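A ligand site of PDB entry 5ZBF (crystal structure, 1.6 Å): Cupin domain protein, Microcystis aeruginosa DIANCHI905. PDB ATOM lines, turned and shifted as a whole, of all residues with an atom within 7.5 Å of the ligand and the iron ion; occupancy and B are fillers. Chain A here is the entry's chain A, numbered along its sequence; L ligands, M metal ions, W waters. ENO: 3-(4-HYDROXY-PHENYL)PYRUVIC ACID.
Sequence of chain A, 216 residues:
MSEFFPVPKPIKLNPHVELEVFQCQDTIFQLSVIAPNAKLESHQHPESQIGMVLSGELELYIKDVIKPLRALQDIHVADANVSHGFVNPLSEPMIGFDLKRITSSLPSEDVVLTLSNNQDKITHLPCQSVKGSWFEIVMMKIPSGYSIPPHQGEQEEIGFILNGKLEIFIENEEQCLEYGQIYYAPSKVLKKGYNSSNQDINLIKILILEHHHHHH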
ATOM      1  N   LEU A  13     -10.579  20.451  -1.786  1.00  0.00           N
ATOM      2  CA  LEU A  13     -10.922  19.040  -1.693  1.00  0.00           C
ATOM      3  C   LEU A  13     -11.225  18.508  -3.061  1.00  0.00           C
ATOM      4  O   LEU A  13     -10.918  17.364  -3.387  1.00  0.00           O
ATOM      5  CB  LEU A  13     -12.107  18.842  -0.757  1.00  0.00           C
ATOM      6  CG  LEU A  13     -12.163  17.523   0.008  1.00  0.00           C
ATOM      7  CD1 LEU A  13     -10.841  17.226   0.708  1.00  0.00           C
ATOM      8  CD2 LEU A  13     -13.309  17.553   1.004  1.00  0.00           C
ATOM      9  N   ASN A  14     -11.861  19.351  -3.861  1.00  0.00           N
ATOM     10  CA  ASN A  14     -12.143  19.043  -5.251  1.00  0.00           C
ATOM     11  C   ASN A  14     -12.481  20.401  -5.843  1.00  0.00           C
ATOM     12  O   ASN A  14     -12.376  21.421  -5.135  1.00  0.00           O
ATOM     13  CB  ASN A  14     -13.296  18.028  -5.357  1.00  0.00           C
ATOM     14  CG  ASN A  14     -14.538  18.458  -4.574  1.00  0.00           C
ATOM     15  OD1 ASN A  14     -15.185  19.442  -4.918  1.00  0.00           O
ATOM     16  ND2 ASN A  14     -14.890  17.695  -3.541  1.00  0.00           N
ATOM     17  N   VAL A  17     -15.011  22.350  -3.419  1.00  0.00           N
ATOM     18  CA  VAL A  17     -14.939  22.512  -1.969  1.00  0.00           C
ATOM     19  C   VAL A  17     -13.585  23.029  -1.514  1.00  0.00           C
ATOM     20  O   VAL A  17     -12.548  22.425  -1.775  1.00  0.00           O
ATOM     21  CB  VAL A  17     -15.215  21.178  -1.228  1.00  0.00           C
ATOM     22  CG1 VAL A  17     -15.138  21.378   0.277  1.00  0.00           C
ATOM     23  CG2 VAL A  17     -16.574  20.623  -1.625  1.00  0.00           C
ATOM     24  N   LEU A  19     -11.610  24.263   2.058  1.00  0.00           N
ATOM     25  CA  LEU A  19     -11.689  24.112   3.506  1.00  0.00           C
ATOM     26  C   LEU A  19     -10.552  24.854   4.213  1.00  0.00           C
ATOM     27  O   LEU A  19      -9.446  24.978   3.663  1.00  0.00           O
ATOM     28  CB  LEU A  19     -11.614  22.645   3.893  1.00  0.00           C
ATOM     29  CG  LEU A  19     -12.628  21.644   3.328  1.00  0.00           C
ATOM     30  CD1 LEU A  19     -12.285  20.246   3.795  1.00  0.00           C
ATOM     31  CD2 LEU A  19     -14.052  21.984   3.731  1.00  0.00           C
ATOM     32  N   GLN A  30     -13.637  22.333  10.649  1.00  0.00           N
ATOM     33  CA  GLN A  30     -13.345  22.999   9.378  1.00  0.00           C
ATOM     34  C   GLN A  30     -14.385  24.015   8.970  1.00  0.00           C
ATOM     35  O   GLN A  30     -15.564  23.829   9.166  1.00  0.00           O
ATOM     36  CB  GLN A  30     -13.132  21.959   8.257  1.00  0.00           C
ATOM     37  CG  GLN A  30     -14.327  21.066   7.993  1.00  0.00           C
ATOM     38  CD  GLN A  30     -13.980  19.832   7.169  1.00  0.00           C
ATOM     39  OE1 GLN A  30     -12.886  19.300   7.250  1.00  0.00           O
ATOM     40  NE2 GLN A  30     -14.940  19.360   6.389  1.00  0.00           N
ATOM     41  N   SER A  32     -15.926  25.665   5.646  1.00  0.00           N
ATOM     42  CA  SER A  32     -16.141  25.194   4.272  1.00  0.00           C
ATOM     43  C   SER A  32     -16.674  26.294   3.369  1.00  0.00           C
ATOM     44  O   SER A  32     -17.479  27.108   3.797  1.00  0.00           O
ATOM     45  CB  SER A  32     -17.167  24.065   4.260  1.00  0.00           C
ATOM     46  OG  SER A  32     -16.636  22.862   4.780  1.00  0.00           O
ATOM     47  N   ILE A  34     -18.443  25.924  -0.327  1.00  0.00           N
ATOM     48  CA  ILE A  34     -18.924  25.052  -1.402  1.00  0.00           C
ATOM     49  C   ILE A  34     -19.419  25.908  -2.571  1.00  0.00           C
ATOM     50  O   ILE A  34     -20.268  26.790  -2.409  1.00  0.00           O
ATOM     51  CB  ILE A  34     -20.024  24.096  -0.921  1.00  0.00           C
ATOM     52  CG1 ILE A  34     -19.483  23.152   0.160  1.00  0.00           C
ATOM     53  CG2 ILE A  34     -20.608  23.298  -2.091  1.00  0.00           C
ATOM     54  CD1 ILE A  34     -20.502  22.179   0.705  1.00  0.00           C
ATOM     55  N   LYS A  39     -22.615  19.745  -6.888  1.00  0.00           N
ATOM     56  CA  LYS A  39     -22.996  18.407  -6.464  1.00  0.00           C
ATOM     57  C   LYS A  39     -21.806  17.742  -5.799  1.00  0.00           C
ATOM     58  O   LYS A  39     -20.738  17.649  -6.388  1.00  0.00           O
ATOM     59  CB  LYS A  39     -23.422  17.545  -7.656  1.00  0.00           C
ATOM     60  CG  LYS A  39     -24.736  17.944  -8.287  1.00  0.00           C
ATOM     61  CD  LYS A  39     -24.981  17.237  -9.597  1.00  0.00           C
ATOM     62  CE  LYS A  39     -25.019  15.733  -9.461  1.00  0.00           C
ATOM     63  NZ  LYS A  39     -25.437  15.109 -10.741  1.00  0.00           N
ATOM     64  N   LEU A  40     -22.011  17.278  -4.568  1.00  0.00           N
ATOM     65  CA  LEU A  40     -20.969  16.592  -3.799  1.00  0.00           C
ATOM     66  C   LEU A  40     -21.355  15.123  -3.680  1.00  0.00           C
ATOM     67  O   LEU A  40     -22.350  14.796  -3.041  1.00  0.00           O
ATOM     68  CB  LEU A  40     -20.851  17.188  -2.397  1.00  0.00           C
ATOM     69  CG  LEU A  40     -19.817  18.279  -2.117  1.00  0.00           C
ATOM     70  CD1 LEU A  40     -19.613  19.211  -3.299  1.00  0.00           C
ATOM     71  CD2 LEU A  40     -20.179  19.061  -0.865  1.00  0.00           C
ATOM     72  N   GLU A  41     -20.563  14.255  -4.310  1.00  0.00           N
ATOM     73  CA  GLU A  41     -20.813  12.822  -4.272  1.00  0.00           C
ATOM     74  C   GLU A  41     -20.799  12.314  -2.842  1.00  0.00           C
ATOM     75  O   GLU A  41     -19.989  12.744  -2.023  1.00  0.00           O
ATOM     76  CB  GLU A  41     -19.769  12.058  -5.093  1.00  0.00           C
ATOM     77  CG  GLU A  41     -20.171  10.632  -5.414  1.00  0.00           C
ATOM     78  N   SER A  42     -21.703  11.387  -2.546  1.00  0.00           N
ATOM     79  CA  SER A  42     -21.774  10.801  -1.213  1.00  0.00           C
ATOM     80  C   SER A  42     -20.462  10.106  -0.876  1.00  0.00           C
ATOM     81  O   SER A  42     -19.832   9.487  -1.750  1.00  0.00           O
ATOM     82  CB  SER A  42     -22.929   9.803  -1.128  1.00  0.00           C
ATOM     83  OG  SER A  42     -24.165  10.421  -1.432  1.00  0.00           O
ATOM     84  N   HIS A  43     -20.063  10.210   0.379  1.00  0.00           N
ATOM     85  CA  HIS A  43     -18.912   9.478   0.875  1.00  0.00           C
ATOM     86  C   HIS A  43     -19.199   8.961   2.261  1.00  0.00           C
ATOM     87  O   HIS A  43     -20.231   9.261   2.846  1.00  0.00           O
ATOM     88  CB  HIS A  43     -17.626  10.314   0.812  1.00  0.00           C
ATOM     89  CG  HIS A  43     -17.556  11.444   1.792  1.00  0.00           C
ATOM     90  ND1 HIS A  43     -16.518  12.352   1.778  1.00  0.00           N
ATOM     91  CD2 HIS A  43     -18.383  11.818   2.804  1.00  0.00           C
ATOM     92  CE1 HIS A  43     -16.695  13.238   2.744  1.00  0.00           C
ATOM     93  NE2 HIS A  43     -17.814  12.925   3.388  1.00  0.00           N
ATOM     94  N   GLN A  44     -18.296   8.138   2.776  1.00  0.00           N
ATOM     95  CA  GLN A  44     -18.376   7.683   4.139  1.00  0.00           C
ATOM     96  C   GLN A  44     -16.994   7.661   4.730  1.00  0.00           C
ATOM     97  O   GLN A  44     -15.995   7.537   4.009  1.00  0.00           O
ATOM     98  CB  GLN A  44     -19.074   6.317   4.231  1.00  0.00           C
ATOM     99  CG  GLN A  44     -18.474   5.223   3.373  1.00  0.00           C
ATOM    100  CD  GLN A  44     -19.475   4.115   3.095  1.00  0.00           C
ATOM    101  OE1 GLN A  44     -19.793   3.844   1.944  1.00  0.00           O
ATOM    102  NE2 GLN A  44     -19.982   3.478   4.139  1.00  0.00           N
ATOM    103  N   HIS A  45     -16.935   7.803   6.045  1.00  0.00           N
ATOM    104  CA  HIS A  45     -15.684   7.752   6.778  1.00  0.00           C
ATOM    105  C   HIS A  45     -15.971   7.376   8.219  1.00  0.00           C
ATOM    106  O   HIS A  45     -17.086   7.598   8.708  1.00  0.00           O
ATOM    107  CB  HIS A  45     -14.966   9.106   6.716  1.00  0.00           C
ATOM    108  CG  HIS A  45     -15.886  10.285   6.765  1.00  0.00           C
ATOM    109  ND1 HIS A  45     -16.577  10.633   7.912  1.00  0.00           N
ATOM    110  CD2 HIS A  45     -16.207  11.193   5.831  1.00  0.00           C
ATOM    111  CE1 HIS A  45     -17.287  11.715   7.668  1.00  0.00           C
ATOM    112  NE2 HIS A  45     -17.086  12.074   6.409  1.00  0.00           N
ATOM    113  N   GLU A  47     -15.024   8.694  10.960  1.00  0.00           N
ATOM    114  CA  GLU A  47     -15.362   9.831  11.821  1.00  0.00           C
ATOM    115  C   GLU A  47     -16.839  10.146  11.705  1.00  0.00           C
ATOM    116  O   GLU A  47     -17.405  10.175  10.604  1.00  0.00           O
ATOM    117  CB  GLU A  47     -14.544  11.062  11.464  1.00  0.00           C
ATOM    118  CG  GLU A  47     -13.043  10.928  11.699  1.00  0.00           C
ATOM    119  CD  GLU A  47     -12.299  10.245  10.565  1.00  0.00           C
ATOM    120  OE1 GLU A  47     -12.898   9.966   9.493  1.00  0.00           O
ATOM    121  OE2 GLU A  47     -11.084   9.975  10.738  1.00  0.00           O
ATOM    122  N   SER A  48     -17.463  10.385  12.862  1.00  0.00           N
ATOM    123  CA  SER A  48     -18.779  10.994  12.917  1.00  0.00           C
ATOM    124  C   SER A  48     -18.658  12.463  12.563  1.00  0.00           C
ATOM    125  O   SER A  48     -17.607  13.079  12.807  1.00  0.00           O
ATOM    126  CB  SER A  48     -19.376  10.881  14.311  1.00  0.00           C
ATOM    127  OG  SER A  48     -19.518   9.525  14.700  1.00  0.00           O
ATOM    128  N   GLN A  49     -19.729  13.024  12.007  1.00  0.00           N
ATOM    129  CA  GLN A  49     -19.693  14.371  11.469  1.00  0.00           C
ATOM    130  C   GLN A  49     -20.978  15.122  11.771  1.00  0.00           C
ATOM    131  O   GLN A  49     -22.081  14.570  11.678  1.00  0.00           O
ATOM    132  CB  GLN A  49     -19.481  14.289   9.949  1.00  0.00           C
ATOM    133  CG  GLN A  49     -19.446  15.623   9.227  1.00  0.00           C
ATOM    134  CD  GLN A  49     -19.347  15.444   7.721  1.00  0.00           C
ATOM    135  OE1 GLN A  49     -20.140  15.994   6.955  1.00  0.00           O
ATOM    136  NE2 GLN A  49     -18.362  14.671   7.307  1.00  0.00           N
ATOM    137  N   HIS A  76     -26.659  19.206  10.433  1.00  0.00           N
ATOM    138  CA  HIS A  76     -26.675  17.858   9.852  1.00  0.00           C
ATOM    139  C   HIS A  76     -25.879  16.940  10.765  1.00  0.00           C
ATOM    140  O   HIS A  76     -24.911  17.378  11.392  1.00  0.00           O
ATOM    141  CB  HIS A  76     -26.173  17.831   8.393  1.00  0.00           C
ATOM    142  CG  HIS A  76     -24.689  17.925   8.241  1.00  0.00           C
ATOM    143  ND1 HIS A  76     -24.048  19.115   7.960  1.00  0.00           N
ATOM    144  CD2 HIS A  76     -23.712  16.985   8.304  1.00  0.00           C
ATOM    145  CE1 HIS A  76     -22.748  18.903   7.875  1.00  0.00           C
ATOM    146  NE2 HIS A  76     -22.521  17.624   8.085  1.00  0.00           N
ATOM    147  N   ALA A  78     -24.167  13.060  10.667  1.00  0.00           N
ATOM    148  CA  ALA A  78     -23.804  11.832   9.949  1.00  0.00           C
ATOM    149  C   ALA A  78     -22.961  10.969  10.877  1.00  0.00           C
ATOM    150  O   ALA A  78     -21.777  11.256  11.107  1.00  0.00           O
ATOM    151  CB  ALA A  78     -23.036  12.161   8.688  1.00  0.00           C
ATOM    152  N   VAL A  82     -21.864   6.446   7.925  1.00  0.00           N
ATOM    153  CA  VAL A  82     -23.162   6.685   7.297  1.00  0.00           C
ATOM    154  C   VAL A  82     -22.880   7.481   6.033  1.00  0.00           C
ATOM    155  O   VAL A  82     -22.245   8.534   6.085  1.00  0.00           O
ATOM    156  CB  VAL A  82     -24.120   7.459   8.219  1.00  0.00           C
ATOM    157  CG1 VAL A  82     -25.391   7.860   7.494  1.00  0.00           C
ATOM    158  CG2 VAL A  82     -24.440   6.629   9.447  1.00  0.00           C
ATOM    159  N   HIS A  84     -23.095  10.006   3.213  1.00  0.00           N
ATOM    160  CA  HIS A  84     -23.697  11.344   3.135  1.00  0.00           C
ATOM    161  C   HIS A  84     -23.113  12.140   1.984  1.00  0.00           C
ATOM    162  O   HIS A  84     -21.905  12.064   1.707  1.00  0.00           O
ATOM    163  CB  HIS A  84     -23.521  12.098   4.446  1.00  0.00           C
ATOM    164  CG  HIS A  84     -22.101  12.236   4.895  1.00  0.00           C
ATOM    165  ND1 HIS A  84     -21.419  11.216   5.520  1.00  0.00           N
ATOM    166  CD2 HIS A  84     -21.251  13.285   4.842  1.00  0.00           C
ATOM    167  CE1 HIS A  84     -20.206  11.623   5.818  1.00  0.00           C
ATOM    168  NE2 HIS A  84     -20.077  12.876   5.421  1.00  0.00           N
ATOM    169  N   GLY A  85     -23.989  12.885   1.326  1.00  0.00           N
ATOM    170  CA  GLY A  85     -23.599  13.776   0.223  1.00  0.00           C
ATOM    171  C   GLY A  85     -24.384  15.059   0.328  1.00  0.00           C
ATOM    172  O   GLY A  85     -25.249  15.193   1.186  1.00  0.00           O
ATOM    173  N   PHE A  86     -24.091  16.002  -0.574  1.00  0.00           N
ATOM    174  CA  PHE A  86     -24.718  17.317  -0.549  1.00  0.00           C
ATOM    175  C   PHE A  86     -24.925  17.888  -1.949  1.00  0.00           C
ATOM    176  O   PHE A  86     -24.180  17.577  -2.887  1.00  0.00           O
ATOM    177  CB  PHE A  86     -23.845  18.324   0.221  1.00  0.00           C
ATOM    178  CG  PHE A  86     -23.568  17.921   1.644  1.00  0.00           C
ATOM    179  CD1 PHE A  86     -24.450  18.240   2.660  1.00  0.00           C
ATOM    180  CD2 PHE A  86     -22.388  17.250   1.977  1.00  0.00           C
ATOM    181  CE1 PHE A  86     -24.190  17.877   3.974  1.00  0.00           C
ATOM    182  CE2 PHE A  86     -22.104  16.891   3.287  1.00  0.00           C
ATOM    183  CZ  PHE A  86     -23.013  17.210   4.291  1.00  0.00           C
ATOM    184  N   ASP A  98     -18.007  22.200   9.673  1.00  0.00           N
ATOM    185  CA  ASP A  98     -18.206  20.813  10.115  1.00  0.00           C
ATOM    186  C   ASP A  98     -17.251  20.495  11.242  1.00  0.00           C
ATOM    187  O   ASP A  98     -16.180  21.096  11.352  1.00  0.00           O
ATOM    188  CB  ASP A  98     -17.899  19.794   9.003  1.00  0.00           C
ATOM    189  CG  ASP A  98     -18.527  20.129   7.674  1.00  0.00           C
ATOM    190  OD1 ASP A  98     -17.782  20.623   6.798  1.00  0.00           O
ATOM    191  OD2 ASP A  98     -19.730  19.876   7.504  1.00  0.00           O
ATOM    192  N   LYS A 100     -15.552  16.828  12.862  1.00  0.00           N
ATOM    193  CA  LYS A 100     -15.391  15.390  12.665  1.00  0.00           C
ATOM    194  C   LYS A 100     -14.566  14.800  13.789  1.00  0.00           C
ATOM    195  O   LYS A 100     -13.571  15.387  14.225  1.00  0.00           O
ATOM    196  CB  LYS A 100     -14.757  15.102  11.302  1.00  0.00           C
ATOM    197  CG  LYS A 100     -15.705  15.401  10.140  1.00  0.00           C
ATOM    198  CD  LYS A 100     -14.965  15.534   8.817  1.00  0.00           C
ATOM    199  CE  LYS A 100     -14.357  14.222   8.387  1.00  0.00           C
ATOM    200  NZ  LYS A 100     -13.911  14.325   6.961  1.00  0.00           N
HETATM  201  O4  ENO L   1     -18.813  15.541   4.540  1.00  0.00           O
HETATM  202  C9  ENO L   1     -17.018  16.763   0.779  1.00  0.00           C
HETATM  203  C8  ENO L   1     -16.951  16.065  -0.418  1.00  0.00           C
HETATM  204  C7  ENO L   1     -17.902  15.082  -0.722  1.00  0.00           C
HETATM  205  C6  ENO L   1     -18.925  14.815   0.184  1.00  0.00           C
HETATM  206  C5  ENO L   1     -18.994  15.527   1.385  1.00  0.00           C
HETATM  207  C4  ENO L   1     -18.045  16.501   1.693  1.00  0.00           C
HETATM  208  O3  ENO L   1     -17.834  14.394  -1.899  1.00  0.00           O
HETATM  209  C3  ENO L   1     -18.140  17.244   3.014  1.00  0.00           C
HETATM  210  C2  ENO L   1     -17.887  16.235   4.128  1.00  0.00           C
HETATM  211  C1  ENO L   1     -16.535  16.062   4.680  1.00  0.00           C
HETATM  212  O2  ENO L   1     -15.652  16.941   4.504  1.00  0.00           O
HETATM  213  O1  ENO L   1     -16.307  15.019   5.333  1.00  0.00           O
HETATM  214 FE    FE M   1     -18.107  13.740   5.405  1.00  0.00          FE
HETATM  215  O   HOH W   1     -12.934  16.031   4.253  1.00  0.00           O
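The iron ion is bound by an oxygen (O4) of the ligand (2.1 Å), the side-chain amide nitrogen (NE2) of Gln 49 (2.1 Å), a ring nitrogen (NE2) of His 84 (2.2 Å), a ring nitrogen (NE2) of His 43 (2.2 Å), a ring nitrogen (NE2) of His 45 (2.2 Å) and an oxygen (O1) of the ligand (2.2 Å).
Residues that only touch the ligand: Leu 13, Leu 40 and Phe 86.
Hydrophobic or aromatic side chains within 4 Å of the ligand: Leu 13, Leu 40, His 43, His 45, His 84 and Phe 86.
An oxygen (O2) of the ligand sits at hydrogen-bond distance from the side-chain amide nitrogen of Gln 30, at 3.1 Å.
The backbone carbonyl oxygen (O) of Glu 41 lies within hydrogen-bond range of an oxygen (O3) of the ligand.
An oxygen (O2) of the ligand lies within salt-bridge range of the side-chain amino group (NZ) of Lys 100 (3.99 Å).
The backbone carbonyl oxygen (O) of Phe 86 sits at hydrogen-bond distance from the backbone NH (N) of Leu 40, 2.8 Å away.
ND1 of His 84 is in hydrogen-bond range of O of Val 82 (2.9 Å).
The backbone NH of Gln 30 lies within hydrogen-bond range of the backbone carbonyl oxygen of Asp 98.
O of Gln 49 lies within hydrogen-bond range of N of Ala 78 (2.8 Å).
O of Glu 47 lies within hydrogen-bond range of ND1 of His 45 (2.9 Å).
A ring nitrogen (NE2) of His 76 lies within hydrogen-bond range of the side-chain amide oxygen of Gln 49, at 3.1 Å.
Within 4 Å of the iron ion: His 43, His 45, Gln 49 and His 84.
Water W1 lies within hydrogen-bond range of an oxygen (O2) of the ligand (2.9 Å) and the side-chain amino group (NZ) of Lys 100 (3.3 Å).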
